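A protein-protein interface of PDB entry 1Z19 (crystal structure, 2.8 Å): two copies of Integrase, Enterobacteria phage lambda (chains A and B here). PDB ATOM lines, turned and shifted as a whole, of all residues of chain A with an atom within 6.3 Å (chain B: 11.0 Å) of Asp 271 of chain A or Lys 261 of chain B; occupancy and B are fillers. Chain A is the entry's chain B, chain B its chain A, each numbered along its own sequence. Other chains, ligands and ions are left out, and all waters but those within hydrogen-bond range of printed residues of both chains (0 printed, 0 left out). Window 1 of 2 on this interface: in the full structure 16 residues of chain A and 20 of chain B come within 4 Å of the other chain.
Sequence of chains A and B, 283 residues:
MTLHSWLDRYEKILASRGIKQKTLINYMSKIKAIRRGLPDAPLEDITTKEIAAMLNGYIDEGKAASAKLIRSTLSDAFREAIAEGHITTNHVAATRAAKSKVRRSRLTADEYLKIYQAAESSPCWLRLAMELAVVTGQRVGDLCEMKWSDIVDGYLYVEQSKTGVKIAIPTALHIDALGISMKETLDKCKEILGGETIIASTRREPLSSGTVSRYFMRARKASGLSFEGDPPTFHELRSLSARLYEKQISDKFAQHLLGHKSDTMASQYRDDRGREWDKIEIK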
ATOM      1  N   ARG A 106      13.314 -25.422   3.062  1.00  0.00           N
ATOM      2  CA  ARG A 106      13.443 -23.967   3.002  1.00  0.00           C
ATOM      3  C   ARG A 106      14.938 -23.625   2.998  1.00  0.00           C
ATOM      4  O   ARG A 106      15.784 -24.505   3.183  1.00  0.00           O
ATOM      5  CB  ARG A 106      12.770 -23.310   4.208  1.00  0.00           C
ATOM      6  CG  ARG A 106      11.242 -23.339   4.216  1.00  0.00           C
ATOM      7  CD  ARG A 106      10.662 -22.448   3.129  1.00  0.00           C
ATOM      8  NE  ARG A 106       9.270 -22.060   3.354  1.00  0.00           N
ATOM      9  CZ  ARG A 106       8.439 -21.692   2.377  1.00  0.00           C
ATOM     10  NH1 ARG A 106       8.861 -21.679   1.122  1.00  0.00           N
ATOM     11  NH2 ARG A 106       7.200 -21.303   2.648  1.00  0.00           N
ATOM     12  N   SER A 239      10.714 -17.127  -0.258  1.00  0.00           N
ATOM     13  CA  SER A 239      10.284 -17.209   1.129  1.00  0.00           C
ATOM     14  C   SER A 239      11.348 -16.587   2.003  1.00  0.00           C
ATOM     15  O   SER A 239      11.034 -15.932   3.000  1.00  0.00           O
ATOM     16  CB  SER A 239      10.088 -18.656   1.578  1.00  0.00           C
ATOM     17  OG  SER A 239      10.177 -18.731   2.998  1.00  0.00           O
ATOM     18  N   ARG A 243      10.702 -13.969   4.693  1.00  0.00           N
ATOM     19  CA  ARG A 243      11.021 -14.128   6.100  1.00  0.00           C
ATOM     20  C   ARG A 243      12.023 -13.092   6.604  1.00  0.00           C
ATOM     21  O   ARG A 243      11.914 -12.615   7.735  1.00  0.00           O
ATOM     22  CB  ARG A 243      11.514 -15.550   6.336  1.00  0.00           C
ATOM     23  CG  ARG A 243      10.420 -16.566   6.064  1.00  0.00           C
ATOM     24  CD  ARG A 243      10.905 -17.978   6.223  1.00  0.00           C
ATOM     25  NE  ARG A 243      11.899 -18.320   5.214  1.00  0.00           N
ATOM     26  CZ  ARG A 243      13.065 -18.883   5.503  1.00  0.00           C
ATOM     27  NH1 ARG A 243      13.373 -19.160   6.762  1.00  0.00           N
ATOM     28  NH2 ARG A 243      13.922 -19.167   4.541  1.00  0.00           N
ATOM     29  N   ALA A 266       0.465 -15.398   2.255  1.00  0.00           N
ATOM     30  CA  ALA A 266       1.470 -14.625   2.982  1.00  0.00           C
ATOM     31  C   ALA A 266       2.015 -15.368   4.199  1.00  0.00           C
ATOM     32  O   ALA A 266       3.230 -15.478   4.385  1.00  0.00           O
ATOM     33  CB  ALA A 266       0.885 -13.276   3.409  1.00  0.00           C
ATOM     34  N   SER A 267       1.118 -15.877   5.034  1.00  0.00           N
ATOM     35  CA  SER A 267       1.545 -16.606   6.223  1.00  0.00           C
ATOM     36  C   SER A 267       2.267 -17.892   5.820  1.00  0.00           C
ATOM     37  O   SER A 267       2.908 -18.533   6.644  1.00  0.00           O
ATOM     38  CB  SER A 267       0.338 -16.925   7.128  1.00  0.00           C
ATOM     39  OG  SER A 267      -0.434 -17.998   6.619  1.00  0.00           O
ATOM     40  N   GLN A 268       2.157 -18.254   4.549  1.00  0.00           N
ATOM     41  CA  GLN A 268       2.843 -19.460   4.082  1.00  0.00           C
ATOM     42  C   GLN A 268       4.267 -19.176   3.687  1.00  0.00           C
ATOM     43  O   GLN A 268       5.156 -19.962   4.007  1.00  0.00           O
ATOM     44  CB  GLN A 268       2.086 -20.071   2.905  1.00  0.00           C
ATOM     45  CG  GLN A 268       1.381 -21.371   3.274  1.00  0.00           C
ATOM     46  CD  GLN A 268       0.623 -21.967   2.104  1.00  0.00           C
ATOM     47  OE1 GLN A 268       1.200 -22.216   1.034  1.00  0.00           O
ATOM     48  NE2 GLN A 268      -0.679 -22.201   2.298  1.00  0.00           N
ATOM     49  N   PTR A 269       4.518 -18.071   2.988  1.00  0.00           N
ATOM     50  CA  PTR A 269       5.885 -17.741   2.622  1.00  0.00           C
ATOM     51  C   PTR A 269       6.636 -17.387   3.890  1.00  0.00           C
ATOM     52  O   PTR A 269       7.853 -17.523   3.976  1.00  0.00           O
ATOM     53  CB  PTR A 269       5.914 -16.587   1.609  1.00  0.00           C
ATOM     54  CG  PTR A 269       5.759 -17.112   0.204  1.00  0.00           C
ATOM     55  CD1 PTR A 269       4.524 -17.538  -0.263  1.00  0.00           C
ATOM     56  CD2 PTR A 269       6.859 -17.196  -0.658  1.00  0.00           C
ATOM     57  CE1 PTR A 269       4.389 -18.075  -1.535  1.00  0.00           C
ATOM     58  CE2 PTR A 269       6.733 -17.738  -1.938  1.00  0.00           C
ATOM     59  CZ  PTR A 269       5.500 -18.196  -2.361  1.00  0.00           C
ATOM     60  OH  PTR A 269       5.310 -18.801  -3.588  1.00  0.00           O
ATOM     61  P   PTR A 269       4.313 -18.386  -4.753  1.00  0.00           P
ATOM     62  O1P PTR A 269       5.087 -18.096  -5.978  1.00  0.00           O
ATOM     63  O2P PTR A 269       3.460 -17.310  -4.190  1.00  0.00           O
ATOM     64  N   ARG A 270       5.895 -16.969   4.907  1.00  0.00           N
ATOM     65  CA  ARG A 270       6.432 -16.561   6.180  1.00  0.00           C
ATOM     66  C   ARG A 270       6.897 -17.761   6.999  1.00  0.00           C
ATOM     67  O   ARG A 270       7.606 -17.600   7.980  1.00  0.00           O
ATOM     68  CB  ARG A 270       5.376 -15.779   6.956  1.00  0.00           C
ATOM     69  CG  ARG A 270       5.865 -15.069   8.205  1.00  0.00           C
ATOM     70  CD  ARG A 270       4.671 -14.583   9.043  1.00  0.00           C
ATOM     71  NE  ARG A 270       3.701 -13.816   8.248  1.00  0.00           N
ATOM     72  CZ  ARG A 270       2.407 -13.690   8.554  1.00  0.00           C
ATOM     73  NH1 ARG A 270       1.906 -14.276   9.640  1.00  0.00           N
ATOM     74  NH2 ARG A 270       1.607 -12.980   7.767  1.00  0.00           N
ATOM     75  N   ASP A 271       6.497 -18.965   6.594  1.00  0.00           N
ATOM     76  CA  ASP A 271       6.861 -20.169   7.347  1.00  0.00           C
ATOM     77  C   ASP A 271       8.188 -20.777   6.913  1.00  0.00           C
ATOM     78  O   ASP A 271       8.449 -20.913   5.710  1.00  0.00           O
ATOM     79  CB  ASP A 271       5.732 -21.196   7.205  1.00  0.00           C
ATOM     80  CG  ASP A 271       5.861 -22.393   8.123  1.00  0.00           C
ATOM     81  OD1 ASP A 271       6.968 -22.653   8.650  1.00  0.00           O
ATOM     82  OD2 ASP A 271       4.865 -23.103   8.280  1.00  0.00           O
ATOM     83  N   ASP A 272       9.035 -21.160   7.876  1.00  0.00           N
ATOM     84  CA  ASP A 272      10.325 -21.741   7.522  1.00  0.00           C
ATOM     85  C   ASP A 272      10.280 -23.269   7.581  1.00  0.00           C
ATOM     86  O   ASP A 272      11.290 -23.933   7.403  1.00  0.00           O
ATOM     87  CB  ASP A 272      11.426 -21.219   8.443  1.00  0.00           C
ATOM     88  CG  ASP A 272      11.527 -21.972   9.738  1.00  0.00           C
ATOM     89  OD1 ASP A 272      10.495 -22.479  10.246  1.00  0.00           O
ATOM     90  OD2 ASP A 272      12.637 -22.040  10.297  1.00  0.00           O
ATOM     91  N   ARG A 273       9.103 -23.795   7.878  1.00  0.00           N
ATOM     92  CA  ARG A 273       8.990 -25.228   7.915  1.00  0.00           C
ATOM     93  C   ARG A 273      10.065 -25.925   8.735  1.00  0.00           C
ATOM     94  O   ARG A 273      10.758 -26.822   8.256  1.00  0.00           O
ATOM     95  CB  ARG A 273       8.942 -25.750   6.480  1.00  0.00           C
ATOM     96  CG  ARG A 273       7.747 -25.194   5.739  1.00  0.00           C
ATOM     97  CD  ARG A 273       7.744 -25.481   4.250  1.00  0.00           C
ATOM     98  NE  ARG A 273       6.465 -25.005   3.685  1.00  0.00           N
ATOM     99  CZ  ARG A 273       6.214 -24.853   2.389  1.00  0.00           C
ATOM    100  NH1 ARG A 273       7.140 -25.126   1.475  1.00  0.00           N
ATOM    101  NH2 ARG A 273       5.023 -24.430   2.026  1.00  0.00           N
ATOM    102  N   GLY A 274      10.215 -25.490   9.984  1.00  0.00           N
ATOM    103  CA  GLY A 274      11.166 -26.072  10.916  1.00  0.00           C
ATOM    104  C   GLY A 274      12.653 -25.892  10.700  1.00  0.00           C
ATOM    105  O   GLY A 274      13.459 -26.429  11.454  1.00  0.00           O
ATOM    106  N   ARG B 139       1.647 -24.112  25.434  1.00  0.00           N
ATOM    107  CA  ARG B 139       0.692 -25.181  25.725  1.00  0.00           C
ATOM    108  C   ARG B 139       1.174 -26.004  26.919  1.00  0.00           C
ATOM    109  O   ARG B 139       2.378 -26.158  27.141  1.00  0.00           O
ATOM    110  CB  ARG B 139       0.514 -26.084  24.504  1.00  0.00           C
ATOM    111  CG  ARG B 139       0.070 -25.354  23.244  1.00  0.00           C
ATOM    112  CD  ARG B 139      -0.560 -26.299  22.216  1.00  0.00           C
ATOM    113  NE  ARG B 139      -1.038 -25.567  21.050  1.00  0.00           N
ATOM    114  CZ  ARG B 139      -0.253 -25.085  20.093  1.00  0.00           C
ATOM    115  NH1 ARG B 139       1.061 -25.268  20.144  1.00  0.00           N
ATOM    116  NH2 ARG B 139      -0.781 -24.383  19.101  1.00  0.00           N
ATOM    117  N   GLU B 159      10.187 -26.292  21.118  1.00  0.00           N
ATOM    118  CA  GLU B 159       9.734 -26.886  19.862  1.00  0.00           C
ATOM    119  C   GLU B 159       8.380 -27.489  20.205  1.00  0.00           C
ATOM    120  O   GLU B 159       8.305 -28.597  20.729  1.00  0.00           O
ATOM    121  CB  GLU B 159      10.652 -27.990  19.371  1.00  0.00           C
ATOM    122  CG  GLU B 159      10.015 -28.718  18.201  1.00  0.00           C
ATOM    123  CD  GLU B 159      10.865 -29.834  17.644  1.00  0.00           C
ATOM    124  OE1 GLU B 159      11.273 -30.713  18.432  1.00  0.00           O
ATOM    125  OE2 GLU B 159      11.112 -29.831  16.417  1.00  0.00           O
ATOM    126  N   GLN B 160       7.318 -26.741  19.920  1.00  0.00           N
ATOM    127  CA  GLN B 160       5.958 -27.148  20.234  1.00  0.00           C
ATOM    128  C   GLN B 160       5.557 -28.503  19.687  1.00  0.00           C
ATOM    129  O   GLN B 160       5.527 -28.731  18.486  1.00  0.00           O
ATOM    130  CB  GLN B 160       4.989 -26.084  19.747  1.00  0.00           C
ATOM    131  CG  GLN B 160       5.425 -24.692  20.112  1.00  0.00           C
ATOM    132  CD  GLN B 160       4.340 -23.687  19.863  1.00  0.00           C
ATOM    133  OE1 GLN B 160       3.599 -23.796  18.886  1.00  0.00           O
ATOM    134  NE2 GLN B 160       4.238 -22.691  20.738  1.00  0.00           N
ATOM    135  N   SER B 161       5.228 -29.398  20.605  1.00  0.00           N
ATOM    136  CA  SER B 161       4.840 -30.749  20.271  1.00  0.00           C
ATOM    137  C   SER B 161       3.665 -30.892  19.334  1.00  0.00           C
ATOM    138  O   SER B 161       3.637 -31.797  18.519  1.00  0.00           O
ATOM    139  CB  SER B 161       4.518 -31.502  21.539  1.00  0.00           C
ATOM    140  OG  SER B 161       3.779 -32.659  21.226  1.00  0.00           O
ATOM    141  N   LYS B 162       2.684 -30.008  19.447  1.00  0.00           N
ATOM    142  CA  LYS B 162       1.496 -30.117  18.618  1.00  0.00           C
ATOM    143  C   LYS B 162       1.662 -29.730  17.169  1.00  0.00           C
ATOM    144  O   LYS B 162       1.070 -30.351  16.300  1.00  0.00           O
ATOM    145  CB  LYS B 162       0.352 -29.276  19.210  1.00  0.00           C
ATOM    146  CG  LYS B 162      -0.961 -29.312  18.388  1.00  0.00           C
ATOM    147  CD  LYS B 162      -2.025 -28.401  18.981  1.00  0.00           C
ATOM    148  CE  LYS B 162      -3.392 -28.619  18.326  1.00  0.00           C
ATOM    149  NZ  LYS B 162      -4.461 -27.790  18.965  1.00  0.00           N
ATOM    150  N   THR B 163       2.470 -28.711  16.908  1.00  0.00           N
ATOM    151  CA  THR B 163       2.625 -28.209  15.552  1.00  0.00           C
ATOM    152  C   THR B 163       4.044 -28.148  14.997  1.00  0.00           C
ATOM    153  O   THR B 163       4.244 -27.765  13.852  1.00  0.00           O
ATOM    154  CB  THR B 163       2.045 -26.813  15.485  1.00  0.00           C
ATOM    155  OG1 THR B 163       2.833 -25.946  16.308  1.00  0.00           O
ATOM    156  CG2 THR B 163       0.619 -26.806  16.014  1.00  0.00           C
ATOM    157  N   GLY B 164       5.033 -28.500  15.803  1.00  0.00           N
ATOM    158  CA  GLY B 164       6.407 -28.450  15.332  1.00  0.00           C
ATOM    159  C   GLY B 164       7.004 -27.052  15.303  1.00  0.00           C
ATOM    160  O   GLY B 164       8.175 -26.867  14.959  1.00  0.00           O
ATOM    161  N   VAL B 165       6.206 -26.054  15.656  1.00  0.00           N
ATOM    162  CA  VAL B 165       6.708 -24.693  15.664  1.00  0.00           C
ATOM    163  C   VAL B 165       7.894 -24.601  16.611  1.00  0.00           C
ATOM    164  O   VAL B 165       7.848 -25.127  17.720  1.00  0.00           O
ATOM    165  CB  VAL B 165       5.613 -23.714  16.099  1.00  0.00           C
ATOM    166  CG1 VAL B 165       6.207 -22.359  16.401  1.00  0.00           C
ATOM    167  CG2 VAL B 165       4.575 -23.600  14.994  1.00  0.00           C
ATOM    168  N   LYS B 166       8.962 -23.951  16.156  1.00  0.00           N
ATOM    169  CA  LYS B 166      10.177 -23.782  16.957  1.00  0.00           C
ATOM    170  C   LYS B 166      10.394 -22.307  17.319  1.00  0.00           C
ATOM    171  O   LYS B 166      10.527 -21.448  16.443  1.00  0.00           O
ATOM    172  CB  LYS B 166      11.379 -24.315  16.185  1.00  0.00           C
ATOM    173  CG  LYS B 166      11.235 -25.779  15.831  1.00  0.00           C
ATOM    174  CD  LYS B 166      12.451 -26.308  15.095  1.00  0.00           C
ATOM    175  CE  LYS B 166      12.217 -27.745  14.690  1.00  0.00           C
ATOM    176  NZ  LYS B 166      13.328 -28.271  13.845  1.00  0.00           N
ATOM    177  N   ILE B 167      10.437 -22.012  18.613  1.00  0.00           N
ATOM    178  CA  ILE B 167      10.607 -20.639  19.034  1.00  0.00           C
ATOM    179  C   ILE B 167      11.637 -20.458  20.132  1.00  0.00           C
ATOM    180  O   ILE B 167      11.948 -21.389  20.870  1.00  0.00           O
ATOM    181  CB  ILE B 167       9.284 -20.070  19.528  1.00  0.00           C
ATOM    182  CG1 ILE B 167       8.758 -20.937  20.665  1.00  0.00           C
ATOM    183  CG2 ILE B 167       8.283 -20.042  18.397  1.00  0.00           C
ATOM    184  CD1 ILE B 167       7.458 -20.450  21.259  1.00  0.00           C
ATOM    185  N   ARG B 238      -3.412 -19.587  28.646  1.00  0.00           N
ATOM    186  CA  ARG B 238      -2.699 -19.289  27.408  1.00  0.00           C
ATOM    187  C   ARG B 238      -3.386 -18.164  26.663  1.00  0.00           C
ATOM    188  O   ARG B 238      -2.739 -17.389  25.968  1.00  0.00           O
ATOM    189  CB  ARG B 238      -2.645 -20.544  26.537  1.00  0.00           C
ATOM    190  CG  ARG B 238      -1.887 -20.431  25.218  1.00  0.00           C
ATOM    191  CD  ARG B 238      -1.874 -21.802  24.551  1.00  0.00           C
ATOM    192  NE  ARG B 238      -1.964 -21.728  23.097  1.00  0.00           N
ATOM    193  CZ  ARG B 238      -0.916 -21.699  22.280  1.00  0.00           C
ATOM    194  NH1 ARG B 238       0.321 -21.740  22.771  1.00  0.00           N
ATOM    195  NH2 ARG B 238      -1.103 -21.631  20.967  1.00  0.00           N
ATOM    196  N   LYS B 252       0.787  -8.384  17.272  1.00  0.00           N
ATOM    197  CA  LYS B 252       1.753  -9.140  16.492  1.00  0.00           C
ATOM    198  C   LYS B 252       2.558 -10.028  17.420  1.00  0.00           C
ATOM    199  O   LYS B 252       2.786 -11.201  17.133  1.00  0.00           O
ATOM    200  CB  LYS B 252       2.684  -8.192  15.732  1.00  0.00           C
ATOM    201  N   PHE B 253       2.986  -9.459  18.536  1.00  0.00           N
ATOM    202  CA  PHE B 253       3.777 -10.197  19.501  1.00  0.00           C
ATOM    203  C   PHE B 253       3.001 -11.359  20.108  1.00  0.00           C
ATOM    204  O   PHE B 253       3.508 -12.467  20.205  1.00  0.00           O
ATOM    205  CB  PHE B 253       4.268  -9.244  20.580  1.00  0.00           C
ATOM    206  CG  PHE B 253       4.917  -9.920  21.727  1.00  0.00           C
ATOM    207  CD1 PHE B 253       4.159 -10.386  22.786  1.00  0.00           C
ATOM    208  CD2 PHE B 253       6.291 -10.090  21.757  1.00  0.00           C
ATOM    209  CE1 PHE B 253       4.762 -11.012  23.866  1.00  0.00           C
ATOM    210  CE2 PHE B 253       6.908 -10.714  22.828  1.00  0.00           C
ATOM    211  CZ  PHE B 253       6.141 -11.178  23.890  1.00  0.00           C
ATOM    212  N   ALA B 254       1.767 -11.115  20.514  1.00  0.00           N
ATOM    213  CA  ALA B 254       0.972 -12.185  21.085  1.00  0.00           C
ATOM    214  C   ALA B 254       0.978 -13.395  20.147  1.00  0.00           C
ATOM    215  O   ALA B 254       1.070 -14.538  20.587  1.00  0.00           O
ATOM    216  CB  ALA B 254      -0.445 -11.711  21.316  1.00  0.00           C
ATOM    217  N   GLN B 255       0.886 -13.136  18.850  1.00  0.00           N
ATOM    218  CA  GLN B 255       0.878 -14.195  17.848  1.00  0.00           C
ATOM    219  C   GLN B 255       2.173 -15.002  17.816  1.00  0.00           C
ATOM    220  O   GLN B 255       2.138 -16.230  17.905  1.00  0.00           O
ATOM    221  CB  GLN B 255       0.609 -13.608  16.453  1.00  0.00           C
ATOM    222  CG  GLN B 255      -0.876 -13.430  16.096  1.00  0.00           C
ATOM    223  CD  GLN B 255      -1.571 -14.755  15.774  1.00  0.00           C
ATOM    224  OE1 GLN B 255      -1.061 -15.551  14.981  1.00  0.00           O
ATOM    225  NE2 GLN B 255      -2.741 -14.990  16.377  1.00  0.00           N
ATOM    226  N   HIS B 256       3.313 -14.327  17.693  1.00  0.00           N
ATOM    227  CA  HIS B 256       4.588 -15.027  17.642  1.00  0.00           C
ATOM    228  C   HIS B 256       4.911 -15.804  18.911  1.00  0.00           C
ATOM    229  O   HIS B 256       5.511 -16.872  18.852  1.00  0.00           O
ATOM    230  CB  HIS B 256       5.728 -14.059  17.344  1.00  0.00           C
ATOM    231  CG  HIS B 256       5.598 -13.360  16.028  1.00  0.00           C
ATOM    232  ND1 HIS B 256       6.680 -12.832  15.356  1.00  0.00           N
ATOM    233  CD2 HIS B 256       4.510 -13.069  15.275  1.00  0.00           C
ATOM    234  CE1 HIS B 256       6.264 -12.245  14.246  1.00  0.00           C
ATOM    235  NE2 HIS B 256       4.950 -12.375  14.174  1.00  0.00           N
ATOM    236  N   LEU B 257       4.530 -15.272  20.061  1.00  0.00           N
ATOM    237  CA  LEU B 257       4.801 -15.967  21.303  1.00  0.00           C
ATOM    238  C   LEU B 257       3.990 -17.258  21.369  1.00  0.00           C
ATOM    239  O   LEU B 257       4.533 -18.301  21.709  1.00  0.00           O
ATOM    240  CB  LEU B 257       4.475 -15.077  22.498  1.00  0.00           C
ATOM    241  CG  LEU B 257       4.764 -15.718  23.856  1.00  0.00           C
ATOM    242  CD1 LEU B 257       6.246 -16.029  23.973  1.00  0.00           C
ATOM    243  CD2 LEU B 257       4.322 -14.777  24.960  1.00  0.00           C
ATOM    244  N   LEU B 258       2.696 -17.205  21.050  1.00  0.00           N
ATOM    245  CA  LEU B 258       1.892 -18.421  21.087  1.00  0.00           C
ATOM    246  C   LEU B 258       2.350 -19.325  19.960  1.00  0.00           C
ATOM    247  O   LEU B 258       2.136 -20.533  19.979  1.00  0.00           O
ATOM    248  CB  LEU B 258       0.397 -18.119  20.937  1.00  0.00           C
ATOM    249  CG  LEU B 258      -0.293 -17.303  22.037  1.00  0.00           C
ATOM    250  CD1 LEU B 258      -1.803 -17.526  21.979  1.00  0.00           C
ATOM    251  CD2 LEU B 258       0.228 -17.715  23.397  1.00  0.00           C
ATOM    252  N   GLY B 259       2.988 -18.722  18.970  1.00  0.00           N
ATOM    253  CA  GLY B 259       3.493 -19.485  17.850  1.00  0.00           C
ATOM    254  C   GLY B 259       2.483 -19.961  16.826  1.00  0.00           C
ATOM    255  O   GLY B 259       2.522 -21.116  16.424  1.00  0.00           O
ATOM    256  N   HIS B 260       1.580 -19.086  16.401  1.00  0.00           N
ATOM    257  CA  HIS B 260       0.596 -19.469  15.397  1.00  0.00           C
ATOM    258  C   HIS B 260       1.131 -19.138  14.013  1.00  0.00           C
ATOM    259  O   HIS B 260       1.578 -18.021  13.768  1.00  0.00           O
ATOM    260  CB  HIS B 260      -0.731 -18.742  15.611  1.00  0.00           C
ATOM    261  CG  HIS B 260      -1.444 -19.144  16.863  1.00  0.00           C
ATOM    262  ND1 HIS B 260      -1.258 -20.370  17.463  1.00  0.00           N
ATOM    263  CD2 HIS B 260      -2.369 -18.495  17.608  1.00  0.00           C
ATOM    264  CE1 HIS B 260      -2.039 -20.460  18.525  1.00  0.00           C
ATOM    265  NE2 HIS B 260      -2.724 -19.337  18.635  1.00  0.00           N
ATOM    266  N   LYS B 261       1.085 -20.121  13.118  1.00  0.00           N
ATOM    267  CA  LYS B 261       1.568 -19.947  11.756  1.00  0.00           C
ATOM    268  C   LYS B 261       0.633 -19.034  10.978  1.00  0.00           C
ATOM    269  O   LYS B 261       0.883 -18.713   9.818  1.00  0.00           O
ATOM    270  CB  LYS B 261       1.665 -21.302  11.040  1.00  0.00           C
ATOM    271  CG  LYS B 261       2.687 -22.262  11.630  1.00  0.00           C
ATOM    272  CD  LYS B 261       2.828 -23.506  10.778  1.00  0.00           C
ATOM    273  CE  LYS B 261       3.948 -24.393  11.291  1.00  0.00           C
ATOM    274  NZ  LYS B 261       4.165 -25.586  10.420  1.00  0.00           N
ATOM    275  N   SER B 262      -0.437 -18.601  11.628  1.00  0.00           N
ATOM    276  CA  SER B 262      -1.410 -17.740  10.979  1.00  0.00           C
ATOM    277  C   SER B 262      -1.716 -16.486  11.787  1.00  0.00           C
ATOM    278  O   SER B 262      -0.950 -16.080  12.654  1.00  0.00           O
ATOM    279  CB  SER B 262      -2.699 -18.531  10.756  1.00  0.00           C
ATOM    280  OG  SER B 262      -3.686 -17.725  10.148  1.00  0.00           O
ATOM    281  N   ASP B 263      -2.843 -15.868  11.466  1.00  0.00           N
ATOM    282  CA  ASP B 263      -3.328 -14.677  12.149  1.00  0.00           C
ATOM    283  C   ASP B 263      -4.808 -14.988  12.319  1.00  0.00           C
ATOM    284  O   ASP B 263      -5.608 -14.131  12.693  1.00  0.00           O
ATOM    285  CB  ASP B 263      -3.137 -13.439  11.270  1.00  0.00           C
ATOM    286  N   THR B 264      -5.140 -16.244  12.027  1.00  0.00           N
ATOM    287  CA  THR B 264      -6.500 -16.766  12.098  1.00  0.00           C
ATOM    288  C   THR B 264      -7.034 -16.936  13.521  1.00  0.00           C
ATOM    289  O   THR B 264      -8.234 -16.781  13.758  1.00  0.00           O
ATOM    290  CB  THR B 264      -6.573 -18.113  11.350  1.00  0.00           C
ATOM    291  N   MET B 265      -6.151 -17.256  14.468  1.00  0.00           N
ATOM    292  CA  MET B 265      -6.573 -17.463  15.851  1.00  0.00           C
ATOM    293  C   MET B 265      -6.066 -16.430  16.840  1.00  0.00           C
ATOM    294  O   MET B 265      -6.538 -16.383  17.977  1.00  0.00           O
ATOM    295  CB  MET B 265      -6.152 -18.850  16.313  1.00  0.00           C
ATOM    296  CG  MET B 265      -6.586 -19.925  15.356  1.00  0.00           C
ATOM    297  SD  MET B 265      -6.612 -21.596  16.221  1.00  0.00           S
ATOM    298  CE  MET B 265      -8.493 -21.750  16.494  1.00  0.00           C
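O of Gly 274 of chain A lies within hydrogen-bond range of NZ of Lys 166 of chain B (3.0 Å).
The side-chain amino group of Lys 261 of chain B lies within salt-bridge range of the side-chain carboxylate of Asp 271 of chain A (3.4 Å).
The side-chain carboxylate of Glu 159 of chain B lies within salt-bridge range of the side-chain amino group of Lys 166 of chain B (3.7 Å).
NE of Arg 106 of chain A lies within hydrogen-bond range of O of Asp 271 of chain A (2.7 Å).
The side-chain carboxylate (OD1) of Asp 271 of chain A sits at hydrogen-bond distance from the backbone NH (N) of Arg 273 of chain A, 2.5 Å away.
OD1 of Asp 272 of chain A is in hydrogen-bond range of N of Gly 274 of chain A (3.0 Å).
Among the printed residues, merely in contact across the chains: Ser 267 of chain A with Lys 261 of chain B (3.3 Å).
Asp 271 of chain A touches one residue of chain B.
Lys 261 of chain B touches just these residues of chain A: Ser 267 and Asp 271.
No residue of chain B comes within 4 Å of Arg 270 of chain A.
Arg 273 of chain A touches none of the printed residues of chain B.
Of the printed residues of chain A, Lys 166 of chain B touches Gly 274.
Of the printed residues of chain B, Gly 274 of chain A touches Lys 166.
The nearest residue of chain A that does not touch Lys 261 of chain B is Arg 270 of chain A (4.6 Å).
The nearest printed residue of chain B that does not touch Gly 274 of chain A is Gly 164 of chain B (5.1 Å).
Of the 25 printed residues of chain B, 2 touch a printed residue of chain A.
Of the 12 printed residues of chain A, 3 touch a printed residue of chain B.
Among the printed residues, Asp or Glu carboxylates within 4 Å of a Lys or Arg side-chain nitrogen of the other chain: Asp 271 of chain A with Lys 261 of chain B (3.4 Å).
No position is printed for both chains.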
